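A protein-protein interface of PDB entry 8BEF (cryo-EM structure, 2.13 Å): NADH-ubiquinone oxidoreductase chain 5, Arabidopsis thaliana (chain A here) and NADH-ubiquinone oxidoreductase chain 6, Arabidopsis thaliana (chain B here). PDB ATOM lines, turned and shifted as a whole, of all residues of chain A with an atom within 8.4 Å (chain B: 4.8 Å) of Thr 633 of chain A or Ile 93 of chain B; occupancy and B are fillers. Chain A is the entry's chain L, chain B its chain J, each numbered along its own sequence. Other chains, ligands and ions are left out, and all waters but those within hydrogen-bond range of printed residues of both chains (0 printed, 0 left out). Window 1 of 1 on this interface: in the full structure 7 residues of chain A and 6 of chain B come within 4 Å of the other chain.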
ATOM      1  N   PHE A 626       6.563  11.314  10.823  1.00  0.00           N
ATOM      2  CA  PHE A 626       5.529  10.700  11.652  1.00  0.00           C
ATOM      3  C   PHE A 626       4.158  11.280  11.335  1.00  0.00           C
ATOM      4  O   PHE A 626       3.163  10.549  11.282  1.00  0.00           O
ATOM      5  CB  PHE A 626       5.874  10.896  13.128  1.00  0.00           C
ATOM      6  CG  PHE A 626       4.990  10.130  14.077  1.00  0.00           C
ATOM      7  CD1 PHE A 626       4.505   8.875  13.746  1.00  0.00           C
ATOM      8  CD2 PHE A 626       4.657  10.664  15.312  1.00  0.00           C
ATOM      9  CE1 PHE A 626       3.700   8.171  14.625  1.00  0.00           C
ATOM     10  CE2 PHE A 626       3.849   9.966  16.195  1.00  0.00           C
ATOM     11  CZ  PHE A 626       3.371   8.719  15.852  1.00  0.00           C
ATOM     12  N   ALA A 627       4.089  12.596  11.119  1.00  0.00           N
ATOM     13  CA  ALA A 627       2.824  13.223  10.756  1.00  0.00           C
ATOM     14  C   ALA A 627       2.293  12.680   9.435  1.00  0.00           C
ATOM     15  O   ALA A 627       1.095  12.403   9.308  1.00  0.00           O
ATOM     16  CB  ALA A 627       2.993  14.739  10.680  1.00  0.00           C
ATOM     17  N   MET A 628       3.168  12.520   8.440  1.00  0.00           N
ATOM     18  CA  MET A 628       2.736  11.966   7.161  1.00  0.00           C
ATOM     19  C   MET A 628       2.227  10.539   7.323  1.00  0.00           C
ATOM     20  O   MET A 628       1.202  10.167   6.741  1.00  0.00           O
ATOM     21  CB  MET A 628       3.883  12.012   6.153  1.00  0.00           C
ATOM     22  CG  MET A 628       4.263  13.411   5.704  1.00  0.00           C
ATOM     23  SD  MET A 628       5.907  13.453   4.967  1.00  0.00           S
ATOM     24  CE  MET A 628       5.615  12.578   3.433  1.00  0.00           C
ATOM     25  N   LEU A 629       2.928   9.731   8.120  1.00  0.00           N
ATOM     26  CA  LEU A 629       2.471   8.374   8.395  1.00  0.00           C
ATOM     27  C   LEU A 629       1.125   8.381   9.109  1.00  0.00           C
ATOM     28  O   LEU A 629       0.229   7.602   8.769  1.00  0.00           O
ATOM     29  CB  LEU A 629       3.519   7.637   9.228  1.00  0.00           C
ATOM     30  CG  LEU A 629       3.311   6.152   9.528  1.00  0.00           C
ATOM     31  CD1 LEU A 629       2.793   5.406   8.309  1.00  0.00           C
ATOM     32  CD2 LEU A 629       4.607   5.540  10.035  1.00  0.00           C
ATOM     33  N   LEU A 630       0.966   9.264  10.096  1.00  0.00           N
ATOM     34  CA  LEU A 630      -0.299   9.354  10.816  1.00  0.00           C
ATOM     35  C   LEU A 630      -1.433   9.773   9.888  1.00  0.00           C
ATOM     36  O   LEU A 630      -2.540   9.228   9.964  1.00  0.00           O
ATOM     37  CB  LEU A 630      -0.164  10.334  11.979  1.00  0.00           C
ATOM     38  CG  LEU A 630       0.530   9.808  13.238  1.00  0.00           C
ATOM     39  CD1 LEU A 630       0.591  10.892  14.302  1.00  0.00           C
ATOM     40  CD2 LEU A 630      -0.159   8.559  13.772  1.00  0.00           C
ATOM     41  N   GLY A 631      -1.178  10.745   9.011  1.00  0.00           N
ATOM     42  CA  GLY A 631      -2.193  11.144   8.051  1.00  0.00           C
ATOM     43  C   GLY A 631      -2.564  10.025   7.097  1.00  0.00           C
ATOM     44  O   GLY A 631      -3.737   9.837   6.772  1.00  0.00           O
ATOM     45  N   LEU A 632      -1.565   9.270   6.634  1.00  0.00           N
ATOM     46  CA  LEU A 632      -1.842   8.113   5.788  1.00  0.00           C
ATOM     47  C   LEU A 632      -2.654   7.062   6.538  1.00  0.00           C
ATOM     48  O   LEU A 632      -3.608   6.496   5.992  1.00  0.00           O
ATOM     49  CB  LEU A 632      -0.532   7.521   5.274  1.00  0.00           C
ATOM     50  CG  LEU A 632      -0.609   6.253   4.425  1.00  0.00           C
ATOM     51  CD1 LEU A 632      -1.280   6.540   3.092  1.00  0.00           C
ATOM     52  CD2 LEU A 632       0.777   5.673   4.212  1.00  0.00           C
ATOM     53  N   THR A 633      -2.296   6.795   7.795  1.00  0.00           N
ATOM     54  CA  THR A 633      -3.041   5.829   8.596  1.00  0.00           C
ATOM     55  C   THR A 633      -4.473   6.291   8.831  1.00  0.00           C
ATOM     56  O   THR A 633      -5.414   5.495   8.732  1.00  0.00           O
ATOM     57  CB  THR A 633      -2.330   5.594   9.928  1.00  0.00           C
ATOM     58  OG1 THR A 633      -0.971   5.215   9.681  1.00  0.00           O
ATOM     59  CG2 THR A 633      -3.027   4.498  10.720  1.00  0.00           C
ATOM     60  N   LEU A 634      -4.654   7.577   9.135  1.00  0.00           N
ATOM     61  CA  LEU A 634      -5.995   8.120   9.317  1.00  0.00           C
ATOM     62  C   LEU A 634      -6.819   7.988   8.044  1.00  0.00           C
ATOM     63  O   LEU A 634      -8.012   7.669   8.097  1.00  0.00           O
ATOM     64  CB  LEU A 634      -5.911   9.583   9.754  1.00  0.00           C
ATOM     65  CG  LEU A 634      -7.190  10.410   9.611  1.00  0.00           C
ATOM     66  CD1 LEU A 634      -8.254   9.931  10.591  1.00  0.00           C
ATOM     67  CD2 LEU A 634      -6.906  11.891   9.802  1.00  0.00           C
ATOM     68  N   PHE A 635      -6.196   8.235   6.890  1.00  0.00           N
ATOM     69  CA  PHE A 635      -6.894   8.112   5.614  1.00  0.00           C
ATOM     70  C   PHE A 635      -7.436   6.702   5.414  1.00  0.00           C
ATOM     71  O   PHE A 635      -8.622   6.512   5.121  1.00  0.00           O
ATOM     72  CB  PHE A 635      -5.951   8.480   4.471  1.00  0.00           C
ATOM     73  CG  PHE A 635      -5.971   9.932   4.106  1.00  0.00           C
ATOM     74  CD1 PHE A 635      -6.482  10.877   4.980  1.00  0.00           C
ATOM     75  CD2 PHE A 635      -5.467  10.354   2.890  1.00  0.00           C
ATOM     76  CE1 PHE A 635      -6.489  12.219   4.641  1.00  0.00           C
ATOM     77  CE2 PHE A 635      -5.475  11.691   2.546  1.00  0.00           C
ATOM     78  CZ  PHE A 635      -5.985  12.624   3.424  1.00  0.00           C
ATOM     79  N   VAL A 636      -6.572   5.698   5.572  1.00  0.00           N
ATOM     80  CA  VAL A 636      -6.992   4.309   5.408  1.00  0.00           C
ATOM     81  C   VAL A 636      -8.061   3.955   6.432  1.00  0.00           C
ATOM     82  O   VAL A 636      -9.086   3.347   6.103  1.00  0.00           O
ATOM     83  CB  VAL A 636      -5.777   3.371   5.515  1.00  0.00           C
ATOM     84  CG1 VAL A 636      -6.224   1.917   5.573  1.00  0.00           C
ATOM     85  CG2 VAL A 636      -4.836   3.597   4.346  1.00  0.00           C
ATOM     86  N   THR A 637      -7.845   4.348   7.687  1.00  0.00           N
ATOM     87  CA  THR A 637      -8.744   3.938   8.760  1.00  0.00           C
ATOM     88  C   THR A 637     -10.144   4.504   8.562  1.00  0.00           C
ATOM     89  O   THR A 637     -11.131   3.761   8.568  1.00  0.00           O
ATOM     90  CB  THR A 637      -8.176   4.368  10.112  1.00  0.00           C
ATOM     91  OG1 THR A 637      -7.201   3.411  10.540  1.00  0.00           O
ATOM     92  CG2 THR A 637      -9.283   4.455  11.156  1.00  0.00           C
ATOM     93  N   PHE A 638     -10.253   5.816   8.366  1.00  0.00           N
ATOM     94  CA  PHE A 638     -11.575   6.428   8.334  1.00  0.00           C
ATOM     95  C   PHE A 638     -12.300   6.111   7.032  1.00  0.00           C
ATOM     96  O   PHE A 638     -13.503   5.836   7.035  1.00  0.00           O
ATOM     97  CB  PHE A 638     -11.472   7.939   8.555  1.00  0.00           C
ATOM     98  CG  PHE A 638     -12.702   8.702   8.137  1.00  0.00           C
ATOM     99  CD1 PHE A 638     -12.863   9.142   6.831  1.00  0.00           C
ATOM    100  CD2 PHE A 638     -13.716   8.947   9.043  1.00  0.00           C
ATOM    101  CE1 PHE A 638     -13.993   9.830   6.447  1.00  0.00           C
ATOM    102  CE2 PHE A 638     -14.855   9.635   8.662  1.00  0.00           C
ATOM    103  CZ  PHE A 638     -14.993  10.077   7.363  1.00  0.00           C
ATOM    104  N   PHE A 639     -11.591   6.151   5.911  1.00  0.00           N
ATOM    105  CA  PHE A 639     -12.248   6.127   4.611  1.00  0.00           C
ATOM    106  C   PHE A 639     -12.438   4.733   4.033  1.00  0.00           C
ATOM    107  O   PHE A 639     -13.121   4.599   3.014  1.00  0.00           O
ATOM    108  CB  PHE A 639     -11.465   6.995   3.627  1.00  0.00           C
ATOM    109  CG  PHE A 639     -12.027   8.374   3.475  1.00  0.00           C
ATOM    110  CD1 PHE A 639     -11.359   9.467   3.991  1.00  0.00           C
ATOM    111  CD2 PHE A 639     -13.211   8.582   2.793  1.00  0.00           C
ATOM    112  CE1 PHE A 639     -11.871  10.737   3.861  1.00  0.00           C
ATOM    113  CE2 PHE A 639     -13.720   9.856   2.648  1.00  0.00           C
ATOM    114  CZ  PHE A 639     -13.047  10.932   3.183  1.00  0.00           C
ATOM    115  N   CYS A 640     -11.849   3.696   4.627  1.00  0.00           N
ATOM    116  CA  CYS A 640     -12.129   2.341   4.170  1.00  0.00           C
ATOM    117  C   CYS A 640     -12.535   1.413   5.310  1.00  0.00           C
ATOM    118  O   CYS A 640     -13.490   0.646   5.160  1.00  0.00           O
ATOM    119  CB  CYS A 640     -10.904   1.804   3.415  1.00  0.00           C
ATOM    120  SG  CYS A 640     -11.277   0.596   2.119  1.00  0.00           S
ATOM    121  N   MET A 641     -11.853   1.472   6.453  1.00  0.00           N
ATOM    122  CA  MET A 641     -12.210   0.699   7.650  1.00  0.00           C
ATOM    123  C   MET A 641     -13.137   1.496   8.565  1.00  0.00           C
ATOM    124  O   MET A 641     -12.833   1.814   9.716  1.00  0.00           O
ATOM    125  CB  MET A 641     -10.954   0.224   8.370  1.00  0.00           C
ATOM    126  CG  MET A 641     -10.224  -0.933   7.692  1.00  0.00           C
ATOM    127  SD  MET A 641     -11.283  -1.971   6.636  1.00  0.00           S
ATOM    128  CE  MET A 641     -10.992  -1.388   4.978  1.00  0.00           C
ATOM    129  N   VAL B  89       3.139   1.980  19.264  1.00  0.00           N
ATOM    130  CA  VAL B  89       2.855   2.746  18.051  1.00  0.00           C
ATOM    131  C   VAL B  89       3.139   1.911  16.809  1.00  0.00           C
ATOM    132  O   VAL B  89       2.421   2.003  15.807  1.00  0.00           O
ATOM    133  CB  VAL B  89       3.637   4.076  18.042  1.00  0.00           C
ATOM    134  CG1 VAL B  89       5.128   3.851  17.826  1.00  0.00           C
ATOM    135  CG2 VAL B  89       3.084   4.997  16.972  1.00  0.00           C
ATOM    136  N   SER B  90       4.185   1.085  16.850  1.00  0.00           N
ATOM    137  CA  SER B  90       4.422   0.156  15.753  1.00  0.00           C
ATOM    138  C   SER B  90       3.361  -0.934  15.716  1.00  0.00           C
ATOM    139  O   SER B  90       3.028  -1.437  14.637  1.00  0.00           O
ATOM    140  CB  SER B  90       5.813  -0.464  15.874  1.00  0.00           C
ATOM    141  OG  SER B  90       5.934  -1.199  17.078  1.00  0.00           O
ATOM    142  N   GLY B  91       2.827  -1.313  16.878  1.00  0.00           N
ATOM    143  CA  GLY B  91       1.794  -2.334  16.907  1.00  0.00           C
ATOM    144  C   GLY B  91       0.516  -1.896  16.217  1.00  0.00           C
ATOM    145  O   GLY B  91      -0.054  -2.643  15.418  1.00  0.00           O
ATOM    146  N   ILE B  92       0.040  -0.685  16.518  1.00  0.00           N
ATOM    147  CA  ILE B  92      -1.182  -0.204  15.882  1.00  0.00           C
ATOM    148  C   ILE B  92      -0.940   0.072  14.402  1.00  0.00           C
ATOM    149  O   ILE B  92      -1.701  -0.381  13.540  1.00  0.00           O
ATOM    150  CB  ILE B  92      -1.726   1.042  16.605  1.00  0.00           C
ATOM    151  CG1 ILE B  92      -1.934   0.755  18.091  1.00  0.00           C
ATOM    152  CG2 ILE B  92      -3.026   1.489  15.976  1.00  0.00           C
ATOM    153  CD1 ILE B  92      -1.280   1.765  19.000  1.00  0.00           C
ATOM    154  N   ILE B  93       0.127   0.806  14.083  1.00  0.00           N
ATOM    155  CA  ILE B  93       0.383   1.150  12.688  1.00  0.00           C
ATOM    156  C   ILE B  93       0.670  -0.108  11.879  1.00  0.00           C
ATOM    157  O   ILE B  93       0.164  -0.277  10.764  1.00  0.00           O
ATOM    158  CB  ILE B  93       1.533   2.169  12.580  1.00  0.00           C
ATOM    159  CG1 ILE B  93       1.166   3.477  13.286  1.00  0.00           C
ATOM    160  CG2 ILE B  93       1.846   2.449  11.126  1.00  0.00           C
ATOM    161  CD1 ILE B  93       0.135   4.300  12.568  1.00  0.00           C
ATOM    162  N   GLY B  94       1.472  -1.017  12.435  1.00  0.00           N
ATOM    163  CA  GLY B  94       1.744  -2.265  11.743  1.00  0.00           C
ATOM    164  C   GLY B  94       0.497  -3.104  11.545  1.00  0.00           C
ATOM    165  O   GLY B  94       0.234  -3.592  10.444  1.00  0.00           O
ATOM    166  N   LEU B  95      -0.302  -3.263  12.605  1.00  0.00           N
ATOM    167  CA  LEU B  95      -1.492  -4.107  12.522  1.00  0.00           C
ATOM    168  C   LEU B  95      -2.496  -3.560  11.514  1.00  0.00           C
ATOM    169  O   LEU B  95      -3.005  -4.303  10.667  1.00  0.00           O
ATOM    170  CB  LEU B  95      -2.140  -4.245  13.897  1.00  0.00           C
ATOM    171  CG  LEU B  95      -3.583  -4.749  13.939  1.00  0.00           C
ATOM    172  CD1 LEU B  95      -3.623  -6.263  13.812  1.00  0.00           C
ATOM    173  CD2 LEU B  95      -4.276  -4.295  15.214  1.00  0.00           C
ATOM    174  N   ILE B  96      -2.796  -2.261  11.591  1.00  0.00           N
ATOM    175  CA  ILE B  96      -3.711  -1.649  10.628  1.00  0.00           C
ATOM    176  C   ILE B  96      -3.210  -1.872   9.211  1.00  0.00           C
ATOM    177  O   ILE B  96      -3.958  -2.307   8.327  1.00  0.00           O
ATOM    178  CB  ILE B  96      -3.892  -0.150  10.923  1.00  0.00           C
ATOM    179  CG1 ILE B  96      -4.498   0.065  12.311  1.00  0.00           C
ATOM    180  CG2 ILE B  96      -4.715   0.514   9.831  1.00  0.00           C
ATOM    181  CD1 ILE B  96      -4.685   1.521  12.669  1.00  0.00           C
ATOM    182  N   PHE B  97      -1.932  -1.582   8.976  1.00  0.00           N
ATOM    183  CA  PHE B  97      -1.341  -1.885   7.682  1.00  0.00           C
ATOM    184  C   PHE B  97      -1.382  -3.382   7.409  1.00  0.00           C
ATOM    185  O   PHE B  97      -1.678  -3.807   6.291  1.00  0.00           O
ATOM    186  CB  PHE B  97       0.093  -1.362   7.625  1.00  0.00           C
ATOM    187  CG  PHE B  97       0.207   0.049   7.120  1.00  0.00           C
ATOM    188  CD1 PHE B  97       0.119   1.118   7.997  1.00  0.00           C
ATOM    189  CD2 PHE B  97       0.407   0.310   5.776  1.00  0.00           C
ATOM    190  CE1 PHE B  97       0.227   2.421   7.546  1.00  0.00           C
ATOM    191  CE2 PHE B  97       0.515   1.613   5.315  1.00  0.00           C
ATOM    192  CZ  PHE B  97       0.423   2.669   6.204  1.00  0.00           C
ATOM    193  N   TRP B  98      -1.114  -4.201   8.428  1.00  0.00           N
ATOM    194  CA  TRP B  98      -1.174  -5.646   8.226  1.00  0.00           C
ATOM    195  C   TRP B  98      -2.577  -6.098   7.836  1.00  0.00           C
ATOM    196  O   TRP B  98      -2.752  -6.807   6.839  1.00  0.00           O
ATOM    197  CB  TRP B  98      -0.721  -6.377   9.483  1.00  0.00           C
ATOM    198  CG  TRP B  98      -0.810  -7.858   9.352  1.00  0.00           C
ATOM    199  CD1 TRP B  98       0.036  -8.678   8.664  1.00  0.00           C
ATOM    200  CD2 TRP B  98      -1.827  -8.701   9.901  1.00  0.00           C
ATOM    201  NE1 TRP B  98      -0.381  -9.980   8.767  1.00  0.00           N
ATOM    202  CE2 TRP B  98      -1.526 -10.021   9.519  1.00  0.00           C
ATOM    203  CE3 TRP B  98      -2.961  -8.466  10.682  1.00  0.00           C
ATOM    204  CZ2 TRP B  98      -2.316 -11.104   9.893  1.00  0.00           C
ATOM    205  CZ3 TRP B  98      -3.745  -9.542  11.052  1.00  0.00           C
ATOM    206  CH2 TRP B  98      -3.418 -10.845  10.658  1.00  0.00           C
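Of the 16 printed residues of chain A, 4 touch a printed residue of chain B.
Printed residues of chain B that touch a printed residue of chain A: Val 89, Ile 93, Ile 96 and Phe 97.
Hydrophobic or aromatic side chains of chain B within 4 Å of the printed part of chain A: Val 89, Ile 93, Ile 96 and Phe 97.
Among the printed residues, 6 pairs touch across the chains.
OG1 of Thr 633 of chain A sits at hydrogen-bond distance from O of Leu 629 of chain A (2.8 Å).
The side-chain hydroxyl (OG1) of Thr 637 of chain A lies close to the backbone carbonyl oxygen (O) of Thr 633 of chain A (3.3 Å).
Of chain B, only Ile 93 (3.2 Å), Ile 96 (3.9 Å) and Phe 97 (3.7 Å) come within 4 Å of Thr 633 of chain A.
Of the printed residues of chain A, Ile 93 of chain B touches Thr 633 (3.2 Å).
Printed residues of chain A within 4 Å of Phe 97 of chain B: Leu 632 and Thr 633.
Printed residues of chain A within 4 Å of Val 89 of chain B: Phe 626.
Of the printed residues of chain B, Thr 637 of chain A touches Ile 96.
Of the printed residues of chain B, Phe 626 of chain A touches Val 89 (3.9 Å).
Of the printed residues of chain A, Ile 96 of chain B touches Thr 633 and Thr 637.
Cys 640 of chain A touches none of the printed residues of chain B.
Among the printed residues, pairs that only touch across the chains: Thr 633 of chain A with Ile 93 of chain B (3.2 Å), Leu 632 of chain A with Phe 97 of chain B (3.6 Å), Thr 633 of chain A with Phe 97 of chain B (3.7 Å), Thr 637 of chain A with Ile 96 of chain B (3.8 Å), Phe 626 of chain A with Val 89 of chain B (3.9 Å) and Thr 633 of chain A with Ile 96 of chain B (3.9 Å).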
